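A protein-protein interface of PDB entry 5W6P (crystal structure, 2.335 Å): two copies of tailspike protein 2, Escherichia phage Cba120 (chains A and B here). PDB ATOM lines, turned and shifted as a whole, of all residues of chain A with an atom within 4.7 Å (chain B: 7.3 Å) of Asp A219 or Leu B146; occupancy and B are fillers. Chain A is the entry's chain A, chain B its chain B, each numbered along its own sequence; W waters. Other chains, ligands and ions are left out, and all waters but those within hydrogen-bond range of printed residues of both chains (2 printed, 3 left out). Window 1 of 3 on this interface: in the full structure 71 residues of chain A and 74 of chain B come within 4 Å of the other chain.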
ATOM      1  N   SER A 169      -5.796   2.143  -8.776  1.00  0.00           N
ATOM      2  CA  SER A 169      -6.816   1.428  -9.534  1.00  0.00           C
ATOM      3  C   SER A 169      -6.283   0.072  -9.977  1.00  0.00           C
ATOM      4  O   SER A 169      -5.072  -0.154 -10.050  1.00  0.00           O
ATOM      5  CB  SER A 169      -7.281   2.223 -10.764  1.00  0.00           C
ATOM      6  OG  SER A 169      -7.672   3.537 -10.415  1.00  0.00           O
ATOM      7  N   LEU A 170      -7.215  -0.833 -10.282  1.00  0.00           N
ATOM      8  CA  LEU A 170      -6.910  -2.070 -10.995  1.00  0.00           C
ATOM      9  C   LEU A 170      -6.068  -3.043 -10.166  1.00  0.00           C
ATOM     10  O   LEU A 170      -5.352  -3.876 -10.721  1.00  0.00           O
ATOM     11  CB  LEU A 170      -6.217  -1.764 -12.329  1.00  0.00           C
ATOM     12  CG  LEU A 170      -7.103  -1.044 -13.356  1.00  0.00           C
ATOM     13  CD1 LEU A 170      -6.277  -0.243 -14.346  1.00  0.00           C
ATOM     14  CD2 LEU A 170      -7.964  -2.041 -14.111  1.00  0.00           C
ATOM     15  N   ILE A 171      -6.152  -2.971  -8.842  1.00  0.00           N
ATOM     16  CA  ILE A 171      -5.451  -3.901  -7.969  1.00  0.00           C
ATOM     17  C   ILE A 171      -6.381  -5.037  -7.553  1.00  0.00           C
ATOM     18  O   ILE A 171      -7.595  -4.993  -7.751  1.00  0.00           O
ATOM     19  CB  ILE A 171      -4.868  -3.198  -6.717  1.00  0.00           C
ATOM     20  CG1 ILE A 171      -5.994  -2.625  -5.855  1.00  0.00           C
ATOM     21  CG2 ILE A 171      -3.846  -2.123  -7.106  1.00  0.00           C
ATOM     22  CD1 ILE A 171      -5.581  -2.336  -4.429  1.00  0.00           C
ATOM     23  N   VAL A 172      -5.799  -6.069  -6.953  1.00  0.00           N
ATOM     24  CA  VAL A 172      -6.542  -7.159  -6.337  1.00  0.00           C
ATOM     25  C   VAL A 172      -6.165  -7.207  -4.865  1.00  0.00           C
ATOM     26  O   VAL A 172      -4.976  -7.147  -4.523  1.00  0.00           O
ATOM     27  CB  VAL A 172      -6.237  -8.513  -7.007  1.00  0.00           C
ATOM     28  CG1 VAL A 172      -6.876  -9.651  -6.210  1.00  0.00           C
ATOM     29  CG2 VAL A 172      -6.727  -8.524  -8.448  1.00  0.00           C
ATOM     30  N   TYR A 208      -6.340   6.971 -18.215  1.00  0.00           N
ATOM     31  CA  TYR A 208      -6.650   5.643 -17.698  1.00  0.00           C
ATOM     32  C   TYR A 208      -6.397   4.603 -18.791  1.00  0.00           C
ATOM     33  O   TYR A 208      -6.698   4.855 -19.963  1.00  0.00           O
ATOM     34  CB  TYR A 208      -8.111   5.596 -17.226  1.00  0.00           C
ATOM     35  CG  TYR A 208      -8.644   4.221 -16.830  1.00  0.00           C
ATOM     36  CD1 TYR A 208      -8.984   3.286 -17.800  1.00  0.00           C
ATOM     37  CD2 TYR A 208      -8.848   3.885 -15.498  1.00  0.00           C
ATOM     38  CE1 TYR A 208      -9.471   2.048 -17.465  1.00  0.00           C
ATOM     39  CE2 TYR A 208      -9.345   2.639 -15.145  1.00  0.00           C
ATOM     40  CZ  TYR A 208      -9.655   1.725 -16.139  1.00  0.00           C
ATOM     41  OH  TYR A 208     -10.153   0.482 -15.824  1.00  0.00           O
ATOM     42  N   ARG A 217     -12.247   5.865 -11.208  1.00  0.00           N
ATOM     43  CA  ARG A 217     -12.350   4.465 -11.641  1.00  0.00           C
ATOM     44  C   ARG A 217     -11.442   3.573 -10.797  1.00  0.00           C
ATOM     45  O   ARG A 217     -10.287   3.322 -11.149  1.00  0.00           O
ATOM     46  CB  ARG A 217     -12.019   4.347 -13.125  1.00  0.00           C
ATOM     47  CG  ARG A 217     -13.056   4.986 -14.036  1.00  0.00           C
ATOM     48  CD  ARG A 217     -12.527   5.179 -15.446  1.00  0.00           C
ATOM     49  NE  ARG A 217     -11.704   6.377 -15.544  1.00  0.00           N
ATOM     50  CZ  ARG A 217     -11.280   6.911 -16.686  1.00  0.00           C
ATOM     51  NH1 ARG A 217     -11.602   6.360 -17.849  1.00  0.00           N
ATOM     52  NH2 ARG A 217     -10.533   8.005 -16.659  1.00  0.00           N
ATOM     53  N   ARG A 218     -11.960   3.094  -9.659  1.00  0.00           N
ATOM     54  CA  ARG A 218     -11.200   2.143  -8.843  1.00  0.00           C
ATOM     55  C   ARG A 218     -10.939   0.849  -9.608  1.00  0.00           C
ATOM     56  O   ARG A 218      -9.815   0.330  -9.617  1.00  0.00           O
ATOM     57  CB  ARG A 218     -11.938   1.842  -7.534  1.00  0.00           C
ATOM     58  CG  ARG A 218     -12.148   3.049  -6.623  1.00  0.00           C
ATOM     59  CD  ARG A 218     -10.904   3.408  -5.823  1.00  0.00           C
ATOM     60  NE  ARG A 218      -9.809   3.894  -6.667  1.00  0.00           N
ATOM     61  CZ  ARG A 218      -9.765   5.103  -7.220  1.00  0.00           C
ATOM     62  NH1 ARG A 218     -10.761   5.966  -7.031  1.00  0.00           N
ATOM     63  NH2 ARG A 218      -8.725   5.456  -7.968  1.00  0.00           N
ATOM     64  N   ASP A 219     -11.972   0.310 -10.249  1.00  0.00           N
ATOM     65  CA  ASP A 219     -11.868  -0.895 -11.076  1.00  0.00           C
ATOM     66  C   ASP A 219     -10.996  -1.956 -10.403  1.00  0.00           C
ATOM     67  O   ASP A 219     -10.058  -2.496 -10.991  1.00  0.00           O
ATOM     68  CB  ASP A 219     -11.324  -0.558 -12.473  1.00  0.00           C
ATOM     69  CG  ASP A 219     -12.222   0.412 -13.251  1.00  0.00           C
ATOM     70  OD1 ASP A 219     -13.149   1.018 -12.669  1.00  0.00           O
ATOM     71  OD2 ASP A 219     -12.004   0.568 -14.464  1.00  0.00           O
ATOM     72  N   LEU A 220     -11.316  -2.268  -9.149  1.00  0.00           N
ATOM     73  CA  LEU A 220     -10.505  -3.192  -8.373  1.00  0.00           C
ATOM     74  C   LEU A 220     -11.387  -4.237  -7.685  1.00  0.00           C
ATOM     75  O   LEU A 220     -12.604  -4.066  -7.550  1.00  0.00           O
ATOM     76  CB  LEU A 220      -9.645  -2.426  -7.363  1.00  0.00           C
ATOM     77  CG  LEU A 220     -10.330  -1.588  -6.292  1.00  0.00           C
ATOM     78  CD1 LEU A 220     -10.676  -2.461  -5.090  1.00  0.00           C
ATOM     79  CD2 LEU A 220      -9.470  -0.391  -5.876  1.00  0.00           C
ATOM     80  N   CYS A 221     -10.750  -5.326  -7.241  1.00  0.00           N
ATOM     81  CA  CYS A 221     -11.436  -6.491  -6.690  1.00  0.00           C
ATOM     82  C   CYS A 221     -10.983  -6.738  -5.261  1.00  0.00           C
ATOM     83  O   CYS A 221      -9.786  -6.922  -5.009  1.00  0.00           O
ATOM     84  CB  CYS A 221     -11.160  -7.741  -7.523  1.00  0.00           C
ATOM     85  SG  CYS A 221     -11.742  -7.655  -9.206  1.00  0.00           S
ATOM     86  N   PHE A 242     -16.079   4.304  -8.615  1.00  0.00           N
ATOM     87  CA  PHE A 242     -16.758   3.385  -9.515  1.00  0.00           C
ATOM     88  C   PHE A 242     -16.054   2.034  -9.526  1.00  0.00           C
ATOM     89  O   PHE A 242     -14.820   1.962  -9.462  1.00  0.00           O
ATOM     90  CB  PHE A 242     -16.802   3.947 -10.937  1.00  0.00           C
ATOM     91  CG  PHE A 242     -17.306   5.356 -11.013  1.00  0.00           C
ATOM     92  CD1 PHE A 242     -18.348   5.780 -10.206  1.00  0.00           C
ATOM     93  CD2 PHE A 242     -16.725   6.264 -11.885  1.00  0.00           C
ATOM     94  CE1 PHE A 242     -18.813   7.084 -10.275  1.00  0.00           C
ATOM     95  CE2 PHE A 242     -17.184   7.572 -11.962  1.00  0.00           C
ATOM     96  CZ  PHE A 242     -18.228   7.982 -11.157  1.00  0.00           C
ATOM     97  N   SER A 243     -16.852   0.965  -9.609  1.00  0.00           N
ATOM     98  CA  SER A 243     -16.352  -0.376  -9.913  1.00  0.00           C
ATOM     99  C   SER A 243     -15.440  -0.920  -8.815  1.00  0.00           C
ATOM    100  O   SER A 243     -14.463  -1.619  -9.095  1.00  0.00           O
ATOM    101  CB  SER A 243     -15.633  -0.398 -11.264  1.00  0.00           C
ATOM    102  OG  SER A 243     -16.470   0.096 -12.297  1.00  0.00           O
ATOM    103  N   GLY B 143      -1.599 -13.510 -12.804  1.00  0.00           N
ATOM    104  CA  GLY B 143      -0.855 -12.293 -12.556  1.00  0.00           C
ATOM    105  C   GLY B 143      -1.042 -11.862 -11.118  1.00  0.00           C
ATOM    106  O   GLY B 143      -1.326 -12.688 -10.240  1.00  0.00           O
ATOM    107  N   SER B 144      -0.912 -10.562 -10.866  1.00  0.00           N
ATOM    108  CA  SER B 144      -1.125 -10.036  -9.525  1.00  0.00           C
ATOM    109  C   SER B 144      -1.922  -8.741  -9.574  1.00  0.00           C
ATOM    110  O   SER B 144      -1.832  -7.925  -8.646  1.00  0.00           O
ATOM    111  CB  SER B 144       0.200  -9.817  -8.804  1.00  0.00           C
ATOM    112  OG  SER B 144       0.895 -11.041  -8.648  1.00  0.00           O
ATOM    113  N   GLY B 145      -2.700  -8.538 -10.635  1.00  0.00           N
ATOM    114  CA  GLY B 145      -3.439  -7.306 -10.802  1.00  0.00           C
ATOM    115  C   GLY B 145      -4.006  -7.167 -12.200  1.00  0.00           C
ATOM    116  O   GLY B 145      -3.548  -7.824 -13.142  1.00  0.00           O
ATOM    117  N   LEU B 146      -5.000  -6.301 -12.348  1.00  0.00           N
ATOM    118  CA  LEU B 146      -5.661  -6.126 -13.631  1.00  0.00           C
ATOM    119  C   LEU B 146      -4.874  -5.245 -14.590  1.00  0.00           C
ATOM    120  O   LEU B 146      -5.339  -5.017 -15.710  1.00  0.00           O
ATOM    121  CB  LEU B 146      -7.060  -5.551 -13.414  1.00  0.00           C
ATOM    122  CG  LEU B 146      -8.111  -6.571 -12.986  1.00  0.00           C
ATOM    123  CD1 LEU B 146      -7.748  -7.204 -11.642  1.00  0.00           C
ATOM    124  CD2 LEU B 146      -9.472  -5.909 -12.913  1.00  0.00           C
ATOM    125  N   HIS B 147      -3.696  -4.758 -14.196  1.00  0.00           N
ATOM    126  CA  HIS B 147      -2.977  -3.807 -15.039  1.00  0.00           C
ATOM    127  C   HIS B 147      -1.492  -4.119 -15.176  1.00  0.00           C
ATOM    128  O   HIS B 147      -1.008  -4.342 -16.290  1.00  0.00           O
ATOM    129  CB  HIS B 147      -3.133  -2.387 -14.500  1.00  0.00           C
ATOM    130  CG  HIS B 147      -2.335  -1.378 -15.259  1.00  0.00           C
ATOM    131  ND1 HIS B 147      -2.758  -0.853 -16.461  1.00  0.00           N
ATOM    132  CD2 HIS B 147      -1.125  -0.823 -15.006  1.00  0.00           C
ATOM    133  CE1 HIS B 147      -1.851  -0.002 -16.906  1.00  0.00           C
ATOM    134  NE2 HIS B 147      -0.854   0.039 -16.039  1.00  0.00           N
ATOM    135  N   TYR B 148      -0.754  -4.143 -14.063  1.00  0.00           N
ATOM    136  CA  TYR B 148       0.705  -4.122 -14.173  1.00  0.00           C
ATOM    137  C   TYR B 148       1.281  -5.464 -14.628  1.00  0.00           C
ATOM    138  O   TYR B 148       2.322  -5.492 -15.299  1.00  0.00           O
ATOM    139  CB  TYR B 148       1.324  -3.674 -12.849  1.00  0.00           C
ATOM    140  CG  TYR B 148       1.734  -4.782 -11.896  1.00  0.00           C
ATOM    141  CD1 TYR B 148       3.017  -5.327 -11.939  1.00  0.00           C
ATOM    142  CD2 TYR B 148       0.856  -5.248 -10.924  1.00  0.00           C
ATOM    143  CE1 TYR B 148       3.402  -6.326 -11.055  1.00  0.00           C
ATOM    144  CE2 TYR B 148       1.234  -6.241 -10.030  1.00  0.00           C
ATOM    145  CZ  TYR B 148       2.501  -6.780 -10.102  1.00  0.00           C
ATOM    146  OH  TYR B 148       2.874  -7.766  -9.219  1.00  0.00           O
ATOM    147  N   SER B 149       0.646  -6.577 -14.282  1.00  0.00           N
ATOM    148  CA  SER B 149       1.000  -7.871 -14.850  1.00  0.00           C
ATOM    149  C   SER B 149       0.048  -8.149 -16.010  1.00  0.00           C
ATOM    150  O   SER B 149      -1.160  -8.285 -15.801  1.00  0.00           O
ATOM    151  CB  SER B 149       0.926  -8.970 -13.790  1.00  0.00           C
ATOM    152  OG  SER B 149      -0.306  -8.919 -13.089  1.00  0.00           O
ATOM    153  N   ARG B 150       0.585  -8.221 -17.228  1.00  0.00           N
ATOM    154  CA  ARG B 150      -0.293  -8.264 -18.391  1.00  0.00           C
ATOM    155  C   ARG B 150       0.482  -8.758 -19.600  1.00  0.00           C
ATOM    156  O   ARG B 150       1.715  -8.722 -19.629  1.00  0.00           O
ATOM    157  CB  ARG B 150      -0.895  -6.882 -18.685  1.00  0.00           C
ATOM    158  CG  ARG B 150       0.153  -5.814 -19.041  1.00  0.00           C
ATOM    159  CD  ARG B 150      -0.485  -4.557 -19.634  1.00  0.00           C
ATOM    160  NE  ARG B 150       0.513  -3.575 -20.050  1.00  0.00           N
ATOM    161  CZ  ARG B 150       1.088  -2.699 -19.231  1.00  0.00           C
ATOM    162  NH1 ARG B 150       0.748  -2.659 -17.949  1.00  0.00           N
ATOM    163  NH2 ARG B 150       1.995  -1.853 -19.698  1.00  0.00           N
ATOM    164  N   ASP B 174      -6.238 -15.797 -14.305  1.00  0.00           N
ATOM    165  CA  ASP B 174      -6.616 -15.027 -13.128  1.00  0.00           C
ATOM    166  C   ASP B 174      -5.716 -13.818 -12.911  1.00  0.00           C
ATOM    167  O   ASP B 174      -4.492 -13.950 -12.818  1.00  0.00           O
ATOM    168  CB  ASP B 174      -6.606 -15.899 -11.865  1.00  0.00           C
ATOM    169  CG  ASP B 174      -7.067 -15.128 -10.636  1.00  0.00           C
ATOM    170  OD1 ASP B 174      -8.265 -14.774 -10.578  1.00  0.00           O
ATOM    171  OD2 ASP B 174      -6.236 -14.846  -9.749  1.00  0.00           O
ATOM    172  N   ALA B 175      -6.343 -12.649 -12.786  1.00  0.00           N
ATOM    173  CA  ALA B 175      -5.700 -11.440 -12.267  1.00  0.00           C
ATOM    174  C   ALA B 175      -4.508 -11.003 -13.130  1.00  0.00           C
ATOM    175  O   ALA B 175      -3.382 -10.835 -12.655  1.00  0.00           O
ATOM    176  CB  ALA B 175      -5.279 -11.642 -10.806  1.00  0.00           C
ATOM    177  N   PHE B 176      -4.785 -10.787 -14.415  1.00  0.00           N
ATOM    178  CA  PHE B 176      -3.813 -10.140 -15.286  1.00  0.00           C
ATOM    179  C   PHE B 176      -4.556  -9.389 -16.384  1.00  0.00           C
ATOM    180  O   PHE B 176      -5.771  -9.527 -16.555  1.00  0.00           O
ATOM    181  CB  PHE B 176      -2.812 -11.141 -15.867  1.00  0.00           C
ATOM    182  CG  PHE B 176      -3.419 -12.163 -16.790  1.00  0.00           C
ATOM    183  CD1 PHE B 176      -3.913 -13.366 -16.291  1.00  0.00           C
ATOM    184  CD2 PHE B 176      -3.462 -11.938 -18.160  1.00  0.00           C
ATOM    185  CE1 PHE B 176      -4.458 -14.322 -17.142  1.00  0.00           C
ATOM    186  CE2 PHE B 176      -3.999 -12.886 -19.020  1.00  0.00           C
ATOM    187  CZ  PHE B 176      -4.503 -14.082 -18.512  1.00  0.00           C
ATOM    188  N   GLY B 177      -3.812  -8.568 -17.115  1.00  0.00           N
ATOM    189  CA  GLY B 177      -4.361  -7.767 -18.192  1.00  0.00           C
ATOM    190  C   GLY B 177      -4.009  -8.306 -19.566  1.00  0.00           C
ATOM    191  O   GLY B 177      -2.979  -8.960 -19.752  1.00  0.00           O
ATOM    192  N   VAL B 178      -4.876  -8.019 -20.532  1.00  0.00           N
ATOM    193  CA  VAL B 178      -4.649  -8.313 -21.943  1.00  0.00           C
ATOM    194  C   VAL B 178      -4.934  -7.009 -22.683  1.00  0.00           C
ATOM    195  O   VAL B 178      -6.100  -6.622 -22.849  1.00  0.00           O
ATOM    196  CB  VAL B 178      -5.540  -9.454 -22.441  1.00  0.00           C
ATOM    197  CG1 VAL B 178      -5.270  -9.768 -23.901  1.00  0.00           C
ATOM    198  CG2 VAL B 178      -5.347 -10.703 -21.554  1.00  0.00           C
ATOM    199  N   TYR B 179      -3.878  -6.320 -23.114  1.00  0.00           N
ATOM    200  CA  TYR B 179      -3.975  -4.974 -23.660  1.00  0.00           C
ATOM    201  C   TYR B 179      -3.634  -4.951 -25.145  1.00  0.00           C
ATOM    202  O   TYR B 179      -2.708  -5.634 -25.596  1.00  0.00           O
ATOM    203  CB  TYR B 179      -3.035  -4.005 -22.929  1.00  0.00           C
ATOM    204  CG  TYR B 179      -3.500  -3.533 -21.565  1.00  0.00           C
ATOM    205  CD1 TYR B 179      -4.552  -4.155 -20.894  1.00  0.00           C
ATOM    206  CD2 TYR B 179      -2.881  -2.452 -20.951  1.00  0.00           C
ATOM    207  CE1 TYR B 179      -4.961  -3.708 -19.647  1.00  0.00           C
ATOM    208  CE2 TYR B 179      -3.284  -2.002 -19.718  1.00  0.00           C
ATOM    209  CZ  TYR B 179      -4.321  -2.628 -19.067  1.00  0.00           C
ATOM    210  OH  TYR B 179      -4.708  -2.157 -17.832  1.00  0.00           O
ATOM    211  N   SER B 223     -10.914 -15.132 -14.630  1.00  0.00           N
ATOM    212  CA  SER B 223     -11.212 -14.546 -13.331  1.00  0.00           C
ATOM    213  C   SER B 223     -10.384 -13.283 -13.138  1.00  0.00           C
ATOM    214  O   SER B 223      -9.148 -13.331 -13.198  1.00  0.00           O
ATOM    215  CB  SER B 223     -10.924 -15.572 -12.229  1.00  0.00           C
ATOM    216  OG  SER B 223     -10.934 -14.986 -10.948  1.00  0.00           O
ATOM    217  N   LYS B 224     -11.062 -12.160 -12.902  1.00  0.00           N
ATOM    218  CA  LYS B 224     -10.399 -10.875 -12.656  1.00  0.00           C
ATOM    219  C   LYS B 224      -9.383 -10.555 -13.753  1.00  0.00           C
ATOM    220  O   LYS B 224      -8.241 -10.178 -13.490  1.00  0.00           O
ATOM    221  CB  LYS B 224      -9.732 -10.868 -11.278  1.00  0.00           C
ATOM    222  CG  LYS B 224     -10.662 -11.288 -10.156  1.00  0.00           C
ATOM    223  CD  LYS B 224     -10.039 -11.059  -8.796  1.00  0.00           C
ATOM    224  CE  LYS B 224     -10.409 -12.176  -7.842  1.00  0.00           C
ATOM    225  NZ  LYS B 224      -9.762 -13.447  -8.287  1.00  0.00           N
ATOM    226  N   VAL B 225      -9.805 -10.743 -15.001  1.00  0.00           N
ATOM    227  CA  VAL B 225      -8.996 -10.420 -16.169  1.00  0.00           C
ATOM    228  C   VAL B 225      -9.493  -9.122 -16.796  1.00  0.00           C
ATOM    229  O   VAL B 225     -10.706  -8.903 -16.942  1.00  0.00           O
ATOM    230  CB  VAL B 225      -9.028 -11.577 -17.181  1.00  0.00           C
ATOM    231  CG1 VAL B 225      -8.460 -11.130 -18.530  1.00  0.00           C
ATOM    232  CG2 VAL B 225      -8.259 -12.778 -16.620  1.00  0.00           C
ATOM    233  N   HIS B 226      -8.552  -8.268 -17.187  1.00  0.00           N
ATOM    234  CA  HIS B 226      -8.840  -6.961 -17.770  1.00  0.00           C
ATOM    235  C   HIS B 226      -8.406  -6.985 -19.235  1.00  0.00           C
ATOM    236  O   HIS B 226      -7.217  -7.126 -19.531  1.00  0.00           O
ATOM    237  CB  HIS B 226      -8.119  -5.861 -16.987  1.00  0.00           C
ATOM    238  CG  HIS B 226      -8.292  -4.485 -17.552  1.00  0.00           C
ATOM    239  ND1 HIS B 226      -7.397  -3.466 -17.305  1.00  0.00           N
ATOM    240  CD2 HIS B 226      -9.260  -3.951 -18.337  1.00  0.00           C
ATOM    241  CE1 HIS B 226      -7.800  -2.367 -17.917  1.00  0.00           C
ATOM    242  NE2 HIS B 226      -8.927  -2.634 -18.552  1.00  0.00           N
ATOM    243  N   ILE B 227      -9.373  -6.884 -20.146  1.00  0.00           N
ATOM    244  CA  ILE B 227      -9.128  -6.844 -21.585  1.00  0.00           C
ATOM    245  C   ILE B 227      -9.391  -5.426 -22.065  1.00  0.00           C
ATOM    246  O   ILE B 227     -10.456  -4.863 -21.786  1.00  0.00           O
ATOM    247  CB  ILE B 227     -10.014  -7.843 -22.349  1.00  0.00           C
ATOM    248  CG1 ILE B 227      -9.832  -9.264 -21.808  1.00  0.00           C
ATOM    249  CG2 ILE B 227      -9.741  -7.767 -23.860  1.00  0.00           C
ATOM    250  CD1 ILE B 227     -10.800 -10.273 -22.427  1.00  0.00           C
ATOM    251  N   SER B 248     -15.799 -11.539 -12.611  1.00  0.00           N
ATOM    252  CA  SER B 248     -15.131 -10.245 -12.440  1.00  0.00           C
ATOM    253  C   SER B 248     -14.251  -9.912 -13.646  1.00  0.00           C
ATOM    254  O   SER B 248     -13.167  -9.340 -13.511  1.00  0.00           O
ATOM    255  CB  SER B 248     -14.317 -10.205 -11.144  1.00  0.00           C
ATOM    256  OG  SER B 248     -15.183 -10.252 -10.019  1.00  0.00           O
ATOM    257  N   LEU B 249     -14.728 -10.276 -14.835  1.00  0.00           N
ATOM    258  CA  LEU B 249     -14.097  -9.829 -16.071  1.00  0.00           C
ATOM    259  C   LEU B 249     -14.359  -8.342 -16.297  1.00  0.00           C
ATOM    260  O   LEU B 249     -15.467  -7.846 -16.073  1.00  0.00           O
ATOM    261  CB  LEU B 249     -14.628 -10.638 -17.252  1.00  0.00           C
ATOM    262  CG  LEU B 249     -14.118 -10.301 -18.650  1.00  0.00           C
ATOM    263  CD1 LEU B 249     -12.682 -10.782 -18.823  1.00  0.00           C
ATOM    264  CD2 LEU B 249     -15.039 -10.911 -19.705  1.00  0.00           C
ATOM    265  N   LEU B 250     -13.327  -7.628 -16.738  1.00  0.00           N
ATOM    266  CA  LEU B 250     -13.414  -6.201 -17.027  1.00  0.00           C
ATOM    267  C   LEU B 250     -12.917  -5.981 -18.445  1.00  0.00           C
ATOM    268  O   LEU B 250     -11.768  -6.316 -18.758  1.00  0.00           O
ATOM    269  CB  LEU B 250     -12.586  -5.375 -16.041  1.00  0.00           C
ATOM    270  CG  LEU B 250     -12.533  -3.861 -16.283  1.00  0.00           C
ATOM    271  CD1 LEU B 250     -13.916  -3.210 -16.100  1.00  0.00           C
ATOM    272  CD2 LEU B 250     -11.498  -3.205 -15.379  1.00  0.00           C
ATOM    273  N   ASN B 252     -12.553  -2.999 -21.456  1.00  0.00           N
ATOM    274  CA  ASN B 252     -12.467  -1.557 -21.656  1.00  0.00           C
ATOM    275  C   ASN B 252     -12.008  -1.264 -23.074  1.00  0.00           C
ATOM    276  O   ASN B 252     -11.234  -2.027 -23.657  1.00  0.00           O
ATOM    277  CB  ASN B 252     -11.455  -0.895 -20.692  1.00  0.00           C
ATOM    278  CG  ASN B 252     -11.997  -0.697 -19.300  1.00  0.00           C
ATOM    279  OD1 ASN B 252     -13.093  -0.165 -19.118  1.00  0.00           O
ATOM    280  ND2 ASN B 252     -11.230  -1.113 -18.298  1.00  0.00           N
ATOM    281  N   GLN B 272     -18.206  -6.558 -16.419  1.00  0.00           N
ATOM    282  CA  GLN B 272     -18.344  -5.154 -16.788  1.00  0.00           C
ATOM    283  C   GLN B 272     -17.712  -4.933 -18.157  1.00  0.00           C
ATOM    284  O   GLN B 272     -16.576  -5.355 -18.395  1.00  0.00           O
ATOM    285  CB  GLN B 272     -17.709  -4.195 -15.765  1.00  0.00           C
ATOM    286  CG  GLN B 272     -17.866  -2.723 -16.225  1.00  0.00           C
ATOM    287  CD  GLN B 272     -17.370  -1.661 -15.235  1.00  0.00           C
ATOM    288  OE1 GLN B 272     -16.739  -1.967 -14.224  1.00  0.00           O
ATOM    289  NE2 GLN B 272     -17.657  -0.398 -15.542  1.00  0.00           N
ATOM    290  N   ASN B 274     -17.153  -1.679 -20.883  1.00  0.00           N
ATOM    291  CA  ASN B 274     -17.218  -0.221 -20.847  1.00  0.00           C
ATOM    292  C   ASN B 274     -16.533   0.377 -22.068  1.00  0.00           C
ATOM    293  O   ASN B 274     -15.345   0.134 -22.302  1.00  0.00           O
ATOM    294  CB  ASN B 274     -16.581   0.331 -19.568  1.00  0.00           C
ATOM    295  CG  ASN B 274     -16.275   1.813 -19.673  1.00  0.00           C
ATOM    296  OD1 ASN B 274     -17.177   2.628 -19.875  1.00  0.00           O
ATOM    297  ND2 ASN B 274     -14.998   2.172 -19.556  1.00  0.00           N
HETATM  298  O   HOH W   1     -12.677   3.548 -18.456  1.00  0.00           O
HETATM  299  O   HOH W   2     -19.474  -0.008 -13.102  1.00  0.00           O
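Asp A219 touches just these residues of chain B: Leu B146 and Leu B250. Leu B146 touches just these residues of chain A: Leu A170 (2.9 Å), Val A172 (3.6 Å) and Asp A219 (3.96 Å). Printed residues of chain A within 4 Å of His B226: Leu A170 (3.5 Å). Of the printed residues of chain B, Val A172 touches Leu B146. Of the printed residues of chain A, Gly B145 touches Leu A170 (3.9 Å). Printed residues of chain B within 4 Å of Leu A170: Gly B145 (3.9 Å), Leu B146 (2.9 Å), His B147 (3.8 Å), His B226 (3.5 Å) and Leu B250 (3.9 Å). Leu B249 touches none of the printed residues of chain A.
The backbone carbonyl oxygen (O) of Leu A170 lies within hydrogen-bond range of the backbone NH (N) of Leu B146 (2.9 Å). ND2 of Asn B252 lies within hydrogen-bond range of OH of Tyr A208 (3.1 Å). OG of Ser A243 is in hydrogen-bond range of OE1 of Gln B272 (2.8 Å).
No position is printed for both chains.
Among the printed residues, pairs that only touch across the chains: Leu A170 with Gly B145, Leu A170 with His B147, Leu A170 with His B226, Leu A170 with Leu B250, Val A172 with Leu B146, Tyr A208 with Leu B250, Asp A219 with Leu B146, Asp A219 with Leu B250 and Cys A221 with Lys B224.
Water W1 bridges the side-chain amide nitrogen (ND2) of Asn B274 and the guanidinium group (NH1) of Arg A217. Water W2 lies within hydrogen-bond range of the side-chain amide nitrogen (NE2) of Gln B272 (3.1 Å) and the side-chain hydroxyl (OG) of Ser A243 (3.1 Å).
The backbone carbonyl oxygen (O) of Asp A219 sits close to the backbone NH (N) of Leu A170 (3.4 Å). The backbone carbonyl oxygen (O) of Ser A243 sits at hydrogen-bond distance from the backbone NH (N) of Leu A220 (3.2 Å). The backbone NH of Gly B145 sits at hydrogen-bond distance from the backbone carbonyl oxygen of Ala B175 (3.1 Å). OD1 of Asp B174 lies within salt-bridge range of NZ of Lys B224, 3.0 Å away. O of Phe B176 is in hydrogen-bond range of N of His B226. The side-chain amide nitrogen of Asn B274 lies within hydrogen-bond range of the side-chain amide oxygen of Asn B252, 3.0 Å away.
Of the 25 printed residues of chain B, 8 touch a printed residue of chain A. Of the 12 printed residues of chain A, 6 touch a printed residue of chain B. Hydrophobic or aromatic side chains of chain A within 4 Å of the printed part of chain B: Leu A170, Val A172 and Tyr A208. Among the printed residues, 12 pairs touch across the chains. Among the printed residues, no Asp or Glu carboxylate lies within 4 Å of a Lys or Arg side-chain nitrogen of the other chain.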
